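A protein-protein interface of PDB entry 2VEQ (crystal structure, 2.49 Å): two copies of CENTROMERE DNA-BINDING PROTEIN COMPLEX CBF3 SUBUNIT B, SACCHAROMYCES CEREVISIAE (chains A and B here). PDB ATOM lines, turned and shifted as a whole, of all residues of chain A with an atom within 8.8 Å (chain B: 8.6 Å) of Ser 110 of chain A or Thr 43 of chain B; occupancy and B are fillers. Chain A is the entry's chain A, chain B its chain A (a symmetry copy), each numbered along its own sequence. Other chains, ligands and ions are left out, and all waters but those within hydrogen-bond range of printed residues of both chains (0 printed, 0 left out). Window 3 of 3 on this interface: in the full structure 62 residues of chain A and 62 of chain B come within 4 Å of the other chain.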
ATOM      1  N   ARG A 103     -37.315  22.458 -16.833  1.00  0.00           N
ATOM      2  CA  ARG A 103     -37.124  23.435 -15.768  1.00  0.00           C
ATOM      3  C   ARG A 103     -37.648  24.829 -16.084  1.00  0.00           C
ATOM      4  O   ARG A 103     -37.629  25.718 -15.232  1.00  0.00           O
ATOM      5  CB  ARG A 103     -35.638  23.505 -15.433  1.00  0.00           C
ATOM      6  CG  ARG A 103     -35.043  22.172 -14.973  1.00  0.00           C
ATOM      7  CD  ARG A 103     -33.523  22.212 -15.011  1.00  0.00           C
ATOM      8  NE  ARG A 103     -33.027  23.571 -14.797  1.00  0.00           N
ATOM      9  CZ  ARG A 103     -32.266  24.240 -15.663  1.00  0.00           C
ATOM     10  NH1 ARG A 103     -31.900  23.674 -16.813  1.00  0.00           N
ATOM     11  NH2 ARG A 103     -31.887  25.486 -15.382  1.00  0.00           N
ATOM     12  N   ASP A 106     -39.854  26.068 -13.412  1.00  0.00           N
ATOM     13  CA  ASP A 106     -39.253  26.193 -12.088  1.00  0.00           C
ATOM     14  C   ASP A 106     -39.061  27.639 -11.640  1.00  0.00           C
ATOM     15  O   ASP A 106     -38.791  28.528 -12.455  1.00  0.00           O
ATOM     16  CB  ASP A 106     -37.899  25.479 -12.064  1.00  0.00           C
ATOM     17  CG  ASP A 106     -38.034  23.971 -12.086  1.00  0.00           C
ATOM     18  OD1 ASP A 106     -39.120  23.472 -12.445  1.00  0.00           O
ATOM     19  OD2 ASP A 106     -37.045  23.283 -11.757  1.00  0.00           O
ATOM     20  N   LYS A 107     -39.207  27.864 -10.336  1.00  0.00           N
ATOM     21  CA  LYS A 107     -39.022  29.190  -9.759  1.00  0.00           C
ATOM     22  C   LYS A 107     -37.609  29.307  -9.191  1.00  0.00           C
ATOM     23  O   LYS A 107     -37.155  30.402  -8.850  1.00  0.00           O
ATOM     24  CB  LYS A 107     -40.062  29.461  -8.664  1.00  0.00           C
ATOM     25  CG  LYS A 107     -41.421  29.919  -9.199  1.00  0.00           C
ATOM     26  CD  LYS A 107     -42.215  30.654  -8.127  1.00  0.00           C
ATOM     27  CE  LYS A 107     -43.437  31.365  -8.705  1.00  0.00           C
ATOM     28  NZ  LYS A 107     -44.436  30.425  -9.302  1.00  0.00           N
ATOM     29  N   ASN A 108     -36.929  28.166  -9.097  1.00  0.00           N
ATOM     30  CA  ASN A 108     -35.553  28.090  -8.604  1.00  0.00           C
ATOM     31  C   ASN A 108     -34.682  27.333  -9.603  1.00  0.00           C
ATOM     32  O   ASN A 108     -35.030  26.233 -10.046  1.00  0.00           O
ATOM     33  CB  ASN A 108     -35.482  27.368  -7.254  1.00  0.00           C
ATOM     34  CG  ASN A 108     -35.919  28.242  -6.091  1.00  0.00           C
ATOM     35  OD1 ASN A 108     -35.856  27.824  -4.932  1.00  0.00           O
ATOM     36  ND2 ASN A 108     -36.367  29.454  -6.390  1.00  0.00           N
ATOM     37  N   HIS A 109     -33.548  27.902  -9.964  1.00  0.00           N
ATOM     38  CA  HIS A 109     -32.622  27.278 -10.906  1.00  0.00           C
ATOM     39  C   HIS A 109     -31.222  27.257 -10.301  1.00  0.00           C
ATOM     40  O   HIS A 109     -30.854  28.156  -9.539  1.00  0.00           O
ATOM     41  CB  HIS A 109     -32.581  28.071 -12.218  1.00  0.00           C
ATOM     42  CG  HIS A 109     -33.831  27.979 -13.033  1.00  0.00           C
ATOM     43  ND1 HIS A 109     -34.813  28.947 -13.003  1.00  0.00           N
ATOM     44  CD2 HIS A 109     -34.277  27.018 -13.877  1.00  0.00           C
ATOM     45  CE1 HIS A 109     -35.811  28.584 -13.788  1.00  0.00           C
ATOM     46  NE2 HIS A 109     -35.511  27.416 -14.331  1.00  0.00           N
ATOM     47  N   SER A 110     -30.439  26.254 -10.622  1.00  0.00           N
ATOM     48  CA  SER A 110     -29.069  26.167 -10.126  1.00  0.00           C
ATOM     49  C   SER A 110     -28.176  26.848 -11.160  1.00  0.00           C
ATOM     50  O   SER A 110     -28.532  26.928 -12.342  1.00  0.00           O
ATOM     51  CB  SER A 110     -28.625  24.709  -9.990  1.00  0.00           C
ATOM     52  OG  SER A 110     -28.417  24.128 -11.271  1.00  0.00           O
ATOM     53  N   VAL A 111     -27.021  27.335 -10.717  1.00  0.00           N
ATOM     54  CA  VAL A 111     -26.073  27.979 -11.613  1.00  0.00           C
ATOM     55  C   VAL A 111     -25.704  26.999 -12.726  1.00  0.00           C
ATOM     56  O   VAL A 111     -25.590  27.379 -13.890  1.00  0.00           O
ATOM     57  CB  VAL A 111     -24.797  28.419 -10.838  1.00  0.00           C
ATOM     58  CG1 VAL A 111     -23.615  28.582 -11.790  1.00  0.00           C
ATOM     59  CG2 VAL A 111     -25.079  29.729 -10.109  1.00  0.00           C
ATOM     60  N   ASP A 112     -25.531  25.735 -12.362  1.00  0.00           N
ATOM     61  CA  ASP A 112     -25.186  24.706 -13.337  1.00  0.00           C
ATOM     62  C   ASP A 112     -26.234  24.656 -14.447  1.00  0.00           C
ATOM     63  O   ASP A 112     -25.907  24.738 -15.631  1.00  0.00           O
ATOM     64  CB  ASP A 112     -25.094  23.346 -12.651  1.00  0.00           C
ATOM     65  CG  ASP A 112     -24.635  22.258 -13.585  1.00  0.00           C
ATOM     66  OD1 ASP A 112     -23.536  22.388 -14.153  1.00  0.00           O
ATOM     67  OD2 ASP A 112     -25.371  21.263 -13.751  1.00  0.00           O
ATOM     68  N   GLY A 113     -27.499  24.523 -14.057  1.00  0.00           N
ATOM     69  CA  GLY A 113     -28.558  24.471 -15.045  1.00  0.00           C
ATOM     70  C   GLY A 113     -28.572  25.705 -15.921  1.00  0.00           C
ATOM     71  O   GLY A 113     -28.749  25.611 -17.141  1.00  0.00           O
ATOM     72  N   LYS A 114     -28.371  26.867 -15.305  1.00  0.00           N
ATOM     73  CA  LYS A 114     -28.379  28.125 -16.038  1.00  0.00           C
ATOM     74  C   LYS A 114     -27.247  28.216 -17.058  1.00  0.00           C
ATOM     75  O   LYS A 114     -27.383  28.882 -18.084  1.00  0.00           O
ATOM     76  CB  LYS A 114     -28.307  29.305 -15.066  1.00  0.00           C
ATOM     77  CG  LYS A 114     -29.442  30.314 -15.237  1.00  0.00           C
ATOM     78  CD  LYS A 114     -30.797  29.632 -15.078  1.00  0.00           C
ATOM     79  CE  LYS A 114     -31.940  30.628 -14.987  1.00  0.00           C
ATOM     80  NZ  LYS A 114     -32.217  31.336 -16.263  1.00  0.00           N
ATOM     81  N   TYR A 115     -26.127  27.554 -16.781  1.00  0.00           N
ATOM     82  CA  TYR A 115     -25.015  27.580 -17.720  1.00  0.00           C
ATOM     83  C   TYR A 115     -25.399  26.787 -18.965  1.00  0.00           C
ATOM     84  O   TYR A 115     -25.106  27.211 -20.081  1.00  0.00           O
ATOM     85  CB  TYR A 115     -23.736  27.008 -17.087  1.00  0.00           C
ATOM     86  CG  TYR A 115     -22.749  28.065 -16.623  1.00  0.00           C
ATOM     87  CD1 TYR A 115     -22.160  28.944 -17.534  1.00  0.00           C
ATOM     88  CD2 TYR A 115     -22.405  28.186 -15.276  1.00  0.00           C
ATOM     89  CE1 TYR A 115     -21.251  29.920 -17.118  1.00  0.00           C
ATOM     90  CE2 TYR A 115     -21.501  29.149 -14.848  1.00  0.00           C
ATOM     91  CZ  TYR A 115     -20.928  30.018 -15.775  1.00  0.00           C
ATOM     92  OH  TYR A 115     -20.043  30.987 -15.349  1.00  0.00           O
ATOM     93  N   TRP A 116     -26.065  25.647 -18.786  1.00  0.00           N
ATOM     94  CA  TRP A 116     -26.484  24.855 -19.940  1.00  0.00           C
ATOM     95  C   TRP A 116     -27.492  25.657 -20.751  1.00  0.00           C
ATOM     96  O   TRP A 116     -27.443  25.652 -21.982  1.00  0.00           O
ATOM     97  CB  TRP A 116     -27.105  23.518 -19.515  1.00  0.00           C
ATOM     98  CG  TRP A 116     -26.105  22.482 -19.060  1.00  0.00           C
ATOM     99  CD1 TRP A 116     -26.042  21.884 -17.827  1.00  0.00           C
ATOM    100  CD2 TRP A 116     -25.020  21.925 -19.829  1.00  0.00           C
ATOM    101  NE1 TRP A 116     -24.988  20.997 -17.786  1.00  0.00           N
ATOM    102  CE2 TRP A 116     -24.347  21.003 -18.998  1.00  0.00           C
ATOM    103  CE3 TRP A 116     -24.558  22.118 -21.138  1.00  0.00           C
ATOM    104  CZ2 TRP A 116     -23.234  20.276 -19.432  1.00  0.00           C
ATOM    105  CZ3 TRP A 116     -23.448  21.390 -21.572  1.00  0.00           C
ATOM    106  CH2 TRP A 116     -22.800  20.483 -20.721  1.00  0.00           C
ATOM    107  N   ASP A 117     -28.397  26.356 -20.064  1.00  0.00           N
ATOM    108  CA  ASP A 117     -29.403  27.167 -20.757  1.00  0.00           C
ATOM    109  C   ASP A 117     -28.717  28.240 -21.591  1.00  0.00           C
ATOM    110  O   ASP A 117     -29.053  28.443 -22.760  1.00  0.00           O
ATOM    111  CB  ASP A 117     -30.339  27.873 -19.777  1.00  0.00           C
ATOM    112  CG  ASP A 117     -31.260  26.922 -19.042  1.00  0.00           C
ATOM    113  OD1 ASP A 117     -31.163  25.685 -19.224  1.00  0.00           O
ATOM    114  OD2 ASP A 117     -32.087  27.441 -18.265  1.00  0.00           O
ATOM    115  N   GLN A 176     -28.720  35.082 -19.445  1.00  0.00           N
ATOM    116  CA  GLN A 176     -28.685  33.869 -18.636  1.00  0.00           C
ATOM    117  C   GLN A 176     -27.301  33.636 -18.016  1.00  0.00           C
ATOM    118  O   GLN A 176     -27.200  33.064 -16.928  1.00  0.00           O
ATOM    119  CB  GLN A 176     -29.164  32.669 -19.468  1.00  0.00           C
ATOM    120  CG  GLN A 176     -30.643  32.824 -19.862  1.00  0.00           C
ATOM    121  CD  GLN A 176     -31.136  31.781 -20.852  1.00  0.00           C
ATOM    122  OE1 GLN A 176     -31.531  30.677 -20.475  1.00  0.00           O
ATOM    123  NE2 GLN A 176     -31.111  32.132 -22.130  1.00  0.00           N
ATOM    124  N   GLN A 179     -27.223  35.622 -15.009  1.00  0.00           N
ATOM    125  CA  GLN A 179     -27.984  34.981 -13.938  1.00  0.00           C
ATOM    126  C   GLN A 179     -27.120  33.919 -13.266  1.00  0.00           C
ATOM    127  O   GLN A 179     -27.427  33.467 -12.162  1.00  0.00           O
ATOM    128  CB  GLN A 179     -29.272  34.347 -14.479  1.00  0.00           C
ATOM    129  CG  GLN A 179     -30.288  35.353 -15.010  1.00  0.00           C
ATOM    130  CD  GLN A 179     -31.546  34.693 -15.530  1.00  0.00           C
ATOM    131  OE1 GLN A 179     -31.482  33.747 -16.311  1.00  0.00           O
ATOM    132  NE2 GLN A 179     -32.701  35.196 -15.111  1.00  0.00           N
ATOM    133  N   CYS A 180     -26.039  33.522 -13.938  1.00  0.00           N
ATOM    134  CA  CYS A 180     -25.110  32.543 -13.378  1.00  0.00           C
ATOM    135  C   CYS A 180     -24.100  33.227 -12.461  1.00  0.00           C
ATOM    136  O   CYS A 180     -23.386  32.546 -11.721  1.00  0.00           O
ATOM    137  CB  CYS A 180     -24.276  31.869 -14.470  1.00  0.00           C
ATOM    138  SG  CYS A 180     -25.083  30.766 -15.607  1.00  0.00           S
ATOM    139  N   HIS A 185     -18.163  32.446 -10.870  1.00  0.00           N
ATOM    140  CA  HIS A 185     -18.168  31.018 -11.173  1.00  0.00           C
ATOM    141  C   HIS A 185     -17.586  30.718 -12.553  1.00  0.00           C
ATOM    142  O   HIS A 185     -18.316  30.446 -13.502  1.00  0.00           O
ATOM    143  CB  HIS A 185     -19.603  30.484 -11.105  1.00  0.00           C
ATOM    144  CG  HIS A 185     -20.306  30.809  -9.823  1.00  0.00           C
ATOM    145  ND1 HIS A 185     -21.458  31.563  -9.777  1.00  0.00           N
ATOM    146  CD2 HIS A 185     -19.992  30.522  -8.537  1.00  0.00           C
ATOM    147  CE1 HIS A 185     -21.821  31.732  -8.518  1.00  0.00           C
ATOM    148  NE2 HIS A 185     -20.947  31.110  -7.745  1.00  0.00           N
ATOM    149  N   ASP A 187     -16.566  28.971 -15.645  1.00  0.00           N
ATOM    150  CA  ASP A 187     -16.969  27.692 -16.212  1.00  0.00           C
ATOM    151  C   ASP A 187     -16.704  27.669 -17.716  1.00  0.00           C
ATOM    152  O   ASP A 187     -16.921  28.662 -18.417  1.00  0.00           O
ATOM    153  CB  ASP A 187     -18.457  27.462 -15.933  1.00  0.00           C
ATOM    154  CG  ASP A 187     -18.899  26.051 -16.249  1.00  0.00           C
ATOM    155  OD1 ASP A 187     -18.905  25.671 -17.440  1.00  0.00           O
ATOM    156  OD2 ASP A 187     -19.235  25.319 -15.298  1.00  0.00           O
ATOM    157  N   ARG A 189     -18.316  26.631 -19.992  1.00  0.00           N
ATOM    158  CA  ARG A 189     -19.481  26.925 -20.811  1.00  0.00           C
ATOM    159  C   ARG A 189     -19.568  28.392 -21.216  1.00  0.00           C
ATOM    160  O   ARG A 189     -20.238  28.730 -22.195  1.00  0.00           O
ATOM    161  CB  ARG A 189     -20.755  26.458 -20.098  1.00  0.00           C
ATOM    162  CG  ARG A 189     -20.921  24.936 -20.201  1.00  0.00           C
ATOM    163  CD  ARG A 189     -21.981  24.401 -19.277  1.00  0.00           C
ATOM    164  NE  ARG A 189     -21.547  24.466 -17.890  1.00  0.00           N
ATOM    165  CZ  ARG A 189     -22.301  24.129 -16.853  1.00  0.00           C
ATOM    166  NH1 ARG A 189     -23.541  23.699 -17.050  1.00  0.00           N
ATOM    167  NH2 ARG A 189     -21.814  24.233 -15.624  1.00  0.00           N
ATOM    168  N   ARG B  40     -16.964  25.553  -4.949  1.00  0.00           N
ATOM    169  CA  ARG B  40     -18.089  25.905  -5.789  1.00  0.00           C
ATOM    170  C   ARG B  40     -18.807  24.689  -6.380  1.00  0.00           C
ATOM    171  O   ARG B  40     -18.331  24.083  -7.348  1.00  0.00           O
ATOM    172  CB  ARG B  40     -17.606  26.811  -6.935  1.00  0.00           C
ATOM    173  CG  ARG B  40     -17.246  28.248  -6.551  1.00  0.00           C
ATOM    174  CD  ARG B  40     -16.186  28.809  -7.498  1.00  0.00           C
ATOM    175  NE  ARG B  40     -14.854  28.287  -7.174  1.00  0.00           N
ATOM    176  CZ  ARG B  40     -14.021  27.718  -8.046  1.00  0.00           C
ATOM    177  NH1 ARG B  40     -14.360  27.582  -9.325  1.00  0.00           N
ATOM    178  NH2 ARG B  40     -12.840  27.274  -7.626  1.00  0.00           N
ATOM    179  N   ASP B  41     -19.930  24.309  -5.787  1.00  0.00           N
ATOM    180  CA  ASP B  41     -20.721  23.212  -6.344  1.00  0.00           C
ATOM    181  C   ASP B  41     -21.843  23.939  -7.081  1.00  0.00           C
ATOM    182  O   ASP B  41     -22.807  24.395  -6.466  1.00  0.00           O
ATOM    183  CB  ASP B  41     -21.327  22.321  -5.255  1.00  0.00           C
ATOM    184  CG  ASP B  41     -22.139  21.170  -5.839  1.00  0.00           C
ATOM    185  OD1 ASP B  41     -22.305  21.126  -7.079  1.00  0.00           O
ATOM    186  OD2 ASP B  41     -22.621  20.311  -5.070  1.00  0.00           O
ATOM    187  N   LEU B  42     -21.703  24.066  -8.394  1.00  0.00           N
ATOM    188  CA  LEU B  42     -22.695  24.778  -9.187  1.00  0.00           C
ATOM    189  C   LEU B  42     -24.063  24.100  -9.258  1.00  0.00           C
ATOM    190  O   LEU B  42     -25.065  24.765  -9.518  1.00  0.00           O
ATOM    191  CB  LEU B  42     -22.159  25.009 -10.603  1.00  0.00           C
ATOM    192  CG  LEU B  42     -20.754  25.612 -10.709  1.00  0.00           C
ATOM    193  CD1 LEU B  42     -20.377  25.781 -12.179  1.00  0.00           C
ATOM    194  CD2 LEU B  42     -20.707  26.954  -9.979  1.00  0.00           C
ATOM    195  N   THR B  43     -24.118  22.788  -9.030  1.00  0.00           N
ATOM    196  CA  THR B  43     -25.404  22.093  -9.085  1.00  0.00           C
ATOM    197  C   THR B  43     -26.230  22.362  -7.834  1.00  0.00           C
ATOM    198  O   THR B  43     -27.401  22.002  -7.773  1.00  0.00           O
ATOM    199  CB  THR B  43     -25.252  20.567  -9.228  1.00  0.00           C
ATOM    200  OG1 THR B  43     -24.804  20.018  -7.987  1.00  0.00           O
ATOM    201  CG2 THR B  43     -24.256  20.229 -10.323  1.00  0.00           C
ATOM    202  N   ARG B  44     -25.619  22.992  -6.836  1.00  0.00           N
ATOM    203  CA  ARG B  44     -26.332  23.319  -5.606  1.00  0.00           C
ATOM    204  C   ARG B  44     -26.133  24.784  -5.228  1.00  0.00           C
ATOM    205  O   ARG B  44     -26.213  25.150  -4.054  1.00  0.00           O
ATOM    206  CB  ARG B  44     -25.883  22.402  -4.459  1.00  0.00           C
ATOM    207  CG  ARG B  44     -26.647  21.077  -4.392  1.00  0.00           C
ATOM    208  CD  ARG B  44     -26.141  20.176  -3.267  1.00  0.00           C
ATOM    209  NE  ARG B  44     -25.076  19.277  -3.709  1.00  0.00           N
ATOM    210  CZ  ARG B  44     -25.275  18.175  -4.431  1.00  0.00           C
ATOM    211  NH1 ARG B  44     -26.504  17.823  -4.793  1.00  0.00           N
ATOM    212  NH2 ARG B  44     -24.242  17.428  -4.802  1.00  0.00           N
ATOM    213  N   THR B  45     -25.874  25.616  -6.236  1.00  0.00           N
ATOM    214  CA  THR B  45     -25.676  27.050  -6.043  1.00  0.00           C
ATOM    215  C   THR B  45     -26.817  27.751  -6.766  1.00  0.00           C
ATOM    216  O   THR B  45     -27.029  27.545  -7.955  1.00  0.00           O
ATOM    217  CB  THR B  45     -24.330  27.531  -6.646  1.00  0.00           C
ATOM    218  OG1 THR B  45     -23.244  26.814  -6.044  1.00  0.00           O
ATOM    219  CG2 THR B  45     -24.136  29.022  -6.413  1.00  0.00           C
ATOM    220  N   PRO B  46     -27.574  28.587  -6.050  1.00  0.00           N
ATOM    221  CA  PRO B  46     -28.694  29.292  -6.680  1.00  0.00           C
ATOM    222  C   PRO B  46     -28.257  30.372  -7.659  1.00  0.00           C
ATOM    223  O   PRO B  46     -27.336  31.136  -7.383  1.00  0.00           O
ATOM    224  CB  PRO B  46     -29.452  29.882  -5.485  1.00  0.00           C
ATOM    225  CG  PRO B  46     -29.091  28.947  -4.348  1.00  0.00           C
ATOM    226  CD  PRO B  46     -27.618  28.735  -4.587  1.00  0.00           C
ATOM    227  N   ALA B  47     -28.935  30.429  -8.801  1.00  0.00           N
ATOM    228  CA  ALA B  47     -28.639  31.432  -9.810  1.00  0.00           C
ATOM    229  C   ALA B  47     -29.237  32.743  -9.322  1.00  0.00           C
ATOM    230  O   ALA B  47     -30.083  32.749  -8.436  1.00  0.00           O
ATOM    231  CB  ALA B  47     -29.259  31.036 -11.139  1.00  0.00           C
ATOM    232  N   ASN B  48     -28.787  33.855  -9.885  1.00  0.00           N
ATOM    233  CA  ASN B  48     -29.319  35.152  -9.499  1.00  0.00           C
ATOM    234  C   ASN B  48     -30.342  35.539 -10.568  1.00  0.00           C
ATOM    235  O   ASN B  48     -30.099  36.439 -11.379  1.00  0.00           O
ATOM    236  CB  ASN B  48     -28.199  36.197  -9.440  1.00  0.00           C
ATOM    237  CG  ASN B  48     -28.499  37.315  -8.453  1.00  0.00           C
ATOM    238  OD1 ASN B  48     -29.580  37.900  -8.469  1.00  0.00           O
ATOM    239  ND2 ASN B  48     -27.539  37.613  -7.585  1.00  0.00           N
ATOM    240  N   LEU B  49     -31.475  34.838 -10.575  1.00  0.00           N
ATOM    241  CA  LEU B  49     -32.545  35.078 -11.547  1.00  0.00           C
ATOM    242  C   LEU B  49     -32.940  36.551 -11.536  1.00  0.00           C
ATOM    243  O   LEU B  49     -33.215  37.164 -12.574  1.00  0.00           O
ATOM    244  CB  LEU B  49     -33.769  34.227 -11.193  1.00  0.00           C
ATOM    245  CG  LEU B  49     -33.528  32.737 -10.940  1.00  0.00           C
ATOM    246  CD1 LEU B  49     -34.823  32.066 -10.520  1.00  0.00           C
ATOM    247  CD2 LEU B  49     -32.978  32.094 -12.196  1.00  0.00           C
ATOM    248  N   LYS B 517     -16.922  18.652 -15.368  1.00  0.00           N
ATOM    249  CA  LYS B 517     -18.342  18.831 -15.072  1.00  0.00           C
ATOM    250  C   LYS B 517     -19.034  19.821 -15.998  1.00  0.00           C
ATOM    251  O   LYS B 517     -20.240  19.713 -16.230  1.00  0.00           O
ATOM    252  CB  LYS B 517     -18.537  19.285 -13.622  1.00  0.00           C
ATOM    253  CG  LYS B 517     -18.179  18.232 -12.577  1.00  0.00           C
ATOM    254  CD  LYS B 517     -18.380  18.777 -11.172  1.00  0.00           C
ATOM    255  CE  LYS B 517     -17.724  17.887 -10.132  1.00  0.00           C
ATOM    256  NZ  LYS B 517     -17.827  18.494  -8.777  1.00  0.00           N
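The backbone carbonyl oxygen (O) of Gln 179 of chain A lies within hydrogen-bond range of the backbone NH (N) of Asn 48 of chain B. N of Val 111 of chain A lies within hydrogen-bond range of O of Thr 45 of chain B. NE2 of Gln 179 of chain A lies within hydrogen-bond range of O of Leu 49 of chain B, 3.3 Å away. N of Asp 112 of chain A sits at hydrogen-bond distance from O of Leu 42 of chain B (3.0 Å). The backbone carbonyl oxygen of His 109 of chain A lies within hydrogen-bond range of the backbone NH of Ala 47 of chain B, at 3.1 Å. N of Val 111 of chain A is in hydrogen-bond range of O of Leu 42 of chain B (3.4 Å).
Of the 11 printed residues of chain B, 7 touch a printed residue of chain A. Printed residues of chain B that touch a printed residue of chain A: Leu 42, Thr 43, Thr 45, Pro 46, Ala 47, Asn 48 and Leu 49. Hydrophobic or aromatic side chains of chain B within 4 Å of the printed part of chain A: Leu 42, Ala 47 and Leu 49. Of the 19 printed residues of chain A, 9 touch a printed residue of chain B. Hydrophobic or aromatic side chains of chain A that line the printed part of chain B: His 109, Val 111 and His 185. Among the printed residues, 19 pairs touch across the chains. Among the printed residues, no Asp or Glu carboxylate lies within 4 Å of a Lys or Arg side-chain nitrogen of the other chain.
The side-chain hydroxyl (OG1) of Thr 45 of chain B is in hydrogen-bond range of the backbone carbonyl oxygen (O) of Asp 41 of chain B, 2.5 Å away. ND1 of His 185 of chain A sits at hydrogen-bond distance from O of Cys 180 of chain A (2.9 Å). OE1 of Gln 179 of chain A sits at hydrogen-bond distance from NZ of Lys 114 of chain A (2.5 Å). The side-chain hydroxyl of Thr 43 of chain B sits at hydrogen-bond distance from the side-chain carboxylate of Asp 41 of chain B, at 2.9 Å. The backbone carbonyl oxygen (O) of Arg 103 of chain A sits at hydrogen-bond distance from a ring nitrogen (NE2) of His 109 of chain A (2.9 Å). The backbone NH (N) of Asp 112 of chain A sits close to the side-chain hydroxyl (OG) of Ser 110 of chain A (3.5 Å).
Ser 110 of chain A touches three residues of chain B. Thr 43 of chain B touches just these residues of chain A: Ser 110 and Asp 112. Of the printed residues of chain B, Asp 187 of chain A touches Leu 42. Of the printed residues of chain B, Gln 179 of chain A touches Ala 47 (3.2 Å), Asn 48 (2.7 Å) and Leu 49 (3.3 Å). Printed residues of chain A within 4 Å of Asn 48 of chain B: Gln 179. Printed residues of chain A within 4 Å of Leu 49 of chain B: Lys 107, His 109, Lys 114 and Gln 179. Of the printed residues of chain A, Ala 47 of chain B touches His 109 (3.1 Å), Val 111 (3.96 Å) and Gln 179 (3.2 Å). The nearest residue of chain B that does not touch Ser 110 of chain A is Ala 47 of chain B (4.3 Å). The nearest printed residue of chain A that does not touch Thr 45 of chain B is His 185 of chain A (4.04 Å).
No position is printed for both chains.
Among the printed residues, merely in contact across the chains: Gln 179 of chain A with Ala 47 of chain B (3.2 Å), Ser 110 of chain A with Thr 45 of chain B (3.3 Å), Lys 107 of chain A with Leu 49 of chain B (3.3 Å), Lys 114 of chain A with Leu 49 of chain B (3.3 Å), Asp 187 of chain A with Leu 42 of chain B (3.4 Å), Ser 110 of chain A with Leu 42 of chain B (3.6 Å), Ser 110 of chain A with Thr 43 of chain B (3.7 Å), His 109 of chain A with Leu 49 of chain B (3.7 Å), Asp 112 of chain A with Thr 43 of chain B (3.8 Å), His 109 of chain A with Pro 46 of chain B (3.8 Å), Val 111 of chain A with Pro 46 of chain B (3.8 Å), His 185 of chain A with Leu 42 of chain B (3.9 Å) and Val 111 of chain A with Ala 47 of chain B (3.96 Å).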
